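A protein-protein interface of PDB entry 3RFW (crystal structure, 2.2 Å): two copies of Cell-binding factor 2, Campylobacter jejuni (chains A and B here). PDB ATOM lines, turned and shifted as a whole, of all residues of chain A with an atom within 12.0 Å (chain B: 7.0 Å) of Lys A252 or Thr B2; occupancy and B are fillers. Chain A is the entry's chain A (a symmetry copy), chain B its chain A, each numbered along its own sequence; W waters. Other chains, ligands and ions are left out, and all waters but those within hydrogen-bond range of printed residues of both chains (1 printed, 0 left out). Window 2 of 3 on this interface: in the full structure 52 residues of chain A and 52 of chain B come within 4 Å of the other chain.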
ATOM      1  N   LYS A 248      14.140   4.691  11.539  1.00  0.00           N
ATOM      2  CA  LYS A 248      15.029   5.512  10.756  1.00  0.00           C
ATOM      3  C   LYS A 248      16.335   4.784  10.453  1.00  0.00           C
ATOM      4  O   LYS A 248      17.188   4.589  11.343  1.00  0.00           O
ATOM      5  CB  LYS A 248      15.334   6.814  11.509  1.00  0.00           C
ATOM      6  N   VAL A 249      16.514   4.475   9.172  1.00  0.00           N
ATOM      7  CA  VAL A 249      17.547   3.589   8.677  1.00  0.00           C
ATOM      8  C   VAL A 249      18.478   4.302   7.693  1.00  0.00           C
ATOM      9  O   VAL A 249      18.035   4.790   6.672  1.00  0.00           O
ATOM     10  CB  VAL A 249      16.898   2.370   7.984  1.00  0.00           C
ATOM     11  CG1 VAL A 249      17.966   1.516   7.277  1.00  0.00           C
ATOM     12  CG2 VAL A 249      16.107   1.532   9.006  1.00  0.00           C
ATOM     13  N   GLU A 250      19.772   4.338   7.983  1.00  0.00           N
ATOM     14  CA  GLU A 250      20.745   4.885   7.049  1.00  0.00           C
ATOM     15  C   GLU A 250      21.786   3.835   6.635  1.00  0.00           C
ATOM     16  O   GLU A 250      22.457   3.256   7.484  1.00  0.00           O
ATOM     17  CB  GLU A 250      21.444   6.114   7.664  1.00  0.00           C
ATOM     18  CG  GLU A 250      20.557   6.970   8.601  1.00  0.00           C
ATOM     19  CD  GLU A 250      19.678   7.956   7.851  1.00  0.00           C
ATOM     20  OE1 GLU A 250      20.083   8.355   6.751  1.00  0.00           O
ATOM     21  N   TYR A 251      21.987   3.655   5.332  1.00  0.00           N
ATOM     22  CA  TYR A 251      22.993   2.711   4.827  1.00  0.00           C
ATOM     23  C   TYR A 251      24.312   3.410   4.546  1.00  0.00           C
ATOM     24  O   TYR A 251      24.345   4.362   3.769  1.00  0.00           O
ATOM     25  CB  TYR A 251      22.502   2.007   3.556  1.00  0.00           C
ATOM     26  CG  TYR A 251      21.436   0.985   3.832  1.00  0.00           C
ATOM     27  CD1 TYR A 251      21.776  -0.286   4.283  1.00  0.00           C
ATOM     28  CD2 TYR A 251      20.097   1.331   3.799  1.00  0.00           C
ATOM     29  CE1 TYR A 251      20.796  -1.220   4.598  1.00  0.00           C
ATOM     30  CE2 TYR A 251      19.104   0.401   4.096  1.00  0.00           C
ATOM     31  CZ  TYR A 251      19.467  -0.874   4.517  1.00  0.00           C
ATOM     32  OH  TYR A 251      18.502  -1.805   4.844  1.00  0.00           O
ATOM     33  N   LYS A 252      25.398   2.892   5.127  1.00  0.00           N
ATOM     34  CA  LYS A 252      26.732   3.458   4.935  1.00  0.00           C
ATOM     35  C   LYS A 252      27.485   2.807   3.775  1.00  0.00           C
ATOM     36  O   LYS A 252      26.885   2.157   2.910  1.00  0.00           O
ATOM     37  CB  LYS A 252      27.554   3.350   6.221  1.00  0.00           C
ATOM     38  N   ALA B   1      33.256  -2.428  11.369  1.00  0.00           N
ATOM     39  CA  ALA B   1      32.893  -1.163  10.662  1.00  0.00           C
ATOM     40  C   ALA B   1      31.379  -1.042  10.525  1.00  0.00           C
ATOM     41  O   ALA B   1      30.657  -2.047  10.432  1.00  0.00           O
ATOM     42  CB  ALA B   1      33.557  -1.099   9.304  1.00  0.00           C
ATOM     43  N   THR B   2      30.914   0.198  10.464  1.00  0.00           N
ATOM     44  CA  THR B   2      29.496   0.471  10.503  1.00  0.00           C
ATOM     45  C   THR B   2      28.953   0.468   9.101  1.00  0.00           C
ATOM     46  O   THR B   2      29.488   1.137   8.233  1.00  0.00           O
ATOM     47  CB  THR B   2      29.248   1.818  11.137  1.00  0.00           C
ATOM     48  OG1 THR B   2      29.633   1.734  12.506  1.00  0.00           O
ATOM     49  CG2 THR B   2      27.777   2.195  11.047  1.00  0.00           C
ATOM     50  N   VAL B   3      27.939  -0.349   8.852  1.00  0.00           N
ATOM     51  CA  VAL B   3      27.420  -0.475   7.486  1.00  0.00           C
ATOM     52  C   VAL B   3      26.034   0.161   7.438  1.00  0.00           C
ATOM     53  O   VAL B   3      25.435   0.297   6.380  1.00  0.00           O
ATOM     54  CB  VAL B   3      27.375  -1.960   7.029  1.00  0.00           C
ATOM     55  CG1 VAL B   3      28.787  -2.479   6.806  1.00  0.00           C
ATOM     56  CG2 VAL B   3      26.646  -2.822   8.072  1.00  0.00           C
ATOM     57  N   ALA B   4      25.494   0.466   8.612  1.00  0.00           N
ATOM     58  CA  ALA B   4      24.171   1.066   8.711  1.00  0.00           C
ATOM     59  C   ALA B   4      23.934   1.562  10.126  1.00  0.00           C
ATOM     60  O   ALA B   4      24.596   1.113  11.053  1.00  0.00           O
ATOM     61  CB  ALA B   4      23.089   0.062   8.303  1.00  0.00           C
ATOM     62  N   THR B   5      22.960   2.460  10.291  1.00  0.00           N
ATOM     63  CA  THR B   5      22.502   2.871  11.612  1.00  0.00           C
ATOM     64  C   THR B   5      21.018   2.687  11.573  1.00  0.00           C
ATOM     65  O   THR B   5      20.393   2.822  10.523  1.00  0.00           O
ATOM     66  CB  THR B   5      22.808   4.383  11.932  1.00  0.00           C
ATOM     67  OG1 THR B   5      22.047   5.224  11.050  1.00  0.00           O
ATOM     68  CG2 THR B   5      24.296   4.704  11.760  1.00  0.00           C
ATOM     69  N   LYS B   9      21.542   3.840  16.053  1.00  0.00           N
ATOM     70  CA  LYS B   9      22.466   2.815  16.497  1.00  0.00           C
ATOM     71  C   LYS B   9      23.158   2.144  15.320  1.00  0.00           C
ATOM     72  O   LYS B   9      22.508   1.645  14.380  1.00  0.00           O
ATOM     73  CB  LYS B   9      21.735   1.773  17.351  1.00  0.00           C
ATOM     74  CG  LYS B   9      22.575   0.512  17.599  1.00  0.00           C
ATOM     75  CD  LYS B   9      21.837  -0.565  18.426  1.00  0.00           C
ATOM     76  CE  LYS B   9      21.275  -1.694  17.527  1.00  0.00           C
ATOM     77  NZ  LYS B   9      22.321  -2.171  16.598  1.00  0.00           N
ATOM     78  N   SER B  10      24.458   1.981  15.474  1.00  0.00           N
ATOM     79  CA  SER B  10      25.329   1.414  14.476  1.00  0.00           C
ATOM     80  C   SER B  10      25.141  -0.095  14.298  1.00  0.00           C
ATOM     81  O   SER B  10      24.949  -0.831  15.259  1.00  0.00           O
ATOM     82  CB  SER B  10      26.783   1.690  14.876  1.00  0.00           C
ATOM     83  OG  SER B  10      27.140   3.004  14.490  1.00  0.00           O
ATOM     84  N   ILE B  11      25.163  -0.534  13.043  1.00  0.00           N
ATOM     85  CA  ILE B  11      25.212  -1.939  12.709  1.00  0.00           C
ATOM     86  C   ILE B  11      26.588  -2.143  12.071  1.00  0.00           C
ATOM     87  O   ILE B  11      26.913  -1.498  11.072  1.00  0.00           O
ATOM     88  CB  ILE B  11      24.081  -2.304  11.689  1.00  0.00           C
ATOM     89  CG1 ILE B  11      22.695  -1.895  12.216  1.00  0.00           C
ATOM     90  CG2 ILE B  11      24.128  -3.772  11.255  1.00  0.00           C
ATOM     91  CD1 ILE B  11      22.116  -2.795  13.322  1.00  0.00           C
ATOM     92  N   SER B  12      27.402  -3.012  12.672  1.00  0.00           N
ATOM     93  CA  SER B  12      28.696  -3.389  12.091  1.00  0.00           C
ATOM     94  C   SER B  12      28.570  -4.420  10.979  1.00  0.00           C
ATOM     95  O   SER B  12      27.602  -5.178  10.934  1.00  0.00           O
ATOM     96  CB  SER B  12      29.630  -3.945  13.166  1.00  0.00           C
ATOM     97  OG  SER B  12      29.042  -5.031  13.869  1.00  0.00           O
ATOM     98  N   ASP B  13      29.606  -4.507  10.148  1.00  0.00           N
ATOM     99  CA  ASP B  13      29.757  -5.607   9.218  1.00  0.00           C
ATOM    100  C   ASP B  13      30.031  -6.927   9.934  1.00  0.00           C
ATOM    101  O   ASP B  13      29.538  -7.984   9.517  1.00  0.00           O
ATOM    102  CB  ASP B  13      30.854  -5.311   8.192  1.00  0.00           C
ATOM    103  CG  ASP B  13      32.208  -5.040   8.837  1.00  0.00           C
ATOM    104  OD1 ASP B  13      32.327  -5.042  10.085  1.00  0.00           O
ATOM    105  OD2 ASP B  13      33.158  -4.812   8.078  1.00  0.00           O
ATOM    106  N   ILE B  41      22.379  -7.034   4.647  1.00  0.00           N
ATOM    107  CA  ILE B  41      22.217  -5.970   5.629  1.00  0.00           C
ATOM    108  C   ILE B  41      20.747  -5.619   5.924  1.00  0.00           C
ATOM    109  O   ILE B  41      20.351  -5.557   7.089  1.00  0.00           O
ATOM    110  CB  ILE B  41      23.033  -4.731   5.281  1.00  0.00           C
ATOM    111  CG1 ILE B  41      24.507  -5.107   5.117  1.00  0.00           C
ATOM    112  CG2 ILE B  41      22.890  -3.695   6.409  1.00  0.00           C
ATOM    113  CD1 ILE B  41      25.371  -3.991   4.553  1.00  0.00           C
HETATM  114  O   HOH W   1      19.584   5.687  11.809  1.00  0.00           O
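N of Thr B5 is in hydrogen-bond range of O of Glu A250 (3.0 Å).
The backbone carbonyl oxygen of Val B3 lies within hydrogen-bond range of the backbone NH of Lys A252 (2.9 Å).
OG1 of Thr B2 lies within hydrogen-bond range of OG of Ser B10, at 3.4 Å.
The backbone carbonyl oxygen (O) of Ala B4 sits at hydrogen-bond distance from the backbone NH (N) of Ile B11 (2.6 Å).
N of Val B3 is in hydrogen-bond range of O of Ile B11.
Among the printed residues, pairs that only touch across the chains: Glu A250 with Ala B4 (3.0 Å), Val A249 with Thr B5 (3.5 Å), Lys A252 with Thr B2 (3.6 Å), Tyr A251 with Ile B41 (3.7 Å), Lys A248 with Thr B5 (3.8 Å) and Tyr A251 with Val B3 (3.8 Å).
Of the printed residues of chain B, Lys A248 touches Thr B5 (3.8 Å).
Of the printed residues of chain B, Tyr A251 touches Val B3 and Ile B41.
Of chain B, only Thr B2 (3.6 Å) and Val B3 (2.9 Å) come within 4 Å of Lys A252.
No residue of chain A comes within 4 Å of Ala B1.
Thr B2 touches just one residue of chain A: Lys A252 (3.6 Å).
Printed residues of chain A within 4 Å of Val B3: Tyr A251 and Lys A252.
Of chain A, only Glu A250 (3.0 Å) comes within 4 Å of Ala B4.
Thr B5 touches three residues of chain A.
No residue of chain A comes within 4 Å of Ile B11.
No residue of chain A comes within 4 Å of Ser B12.
Of the printed residues of chain A, Ile B41 touches Tyr A251.
The nearest residue of chain B that does not touch Lys A252 is Ala B4 (4.2 Å).
The nearest residue of chain A that does not touch Thr B2 is Glu A250 (6.5 Å).
The nearest printed residue of chain B that does not touch Glu A250 is Val B3 (4.3 Å).
Of the 11 printed residues of chain B, 5 touch a printed residue of chain A.
Hydrophobic or aromatic side chains of chain B within 4 Å of the printed part of chain A: Ala B4 and Ile B41.
Hydrophobic or aromatic side chains of chain A within 4 Å of the printed part of chain B: Tyr A251.
No position is printed for both chains.
Of the 8 pairs that touch across the chains among the printed residues, none has its exchanged pair printed and touching as well.
Water W1 bridges the side-chain hydroxyl of Thr B5 and the backbone carbonyl oxygen of Lys A248.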
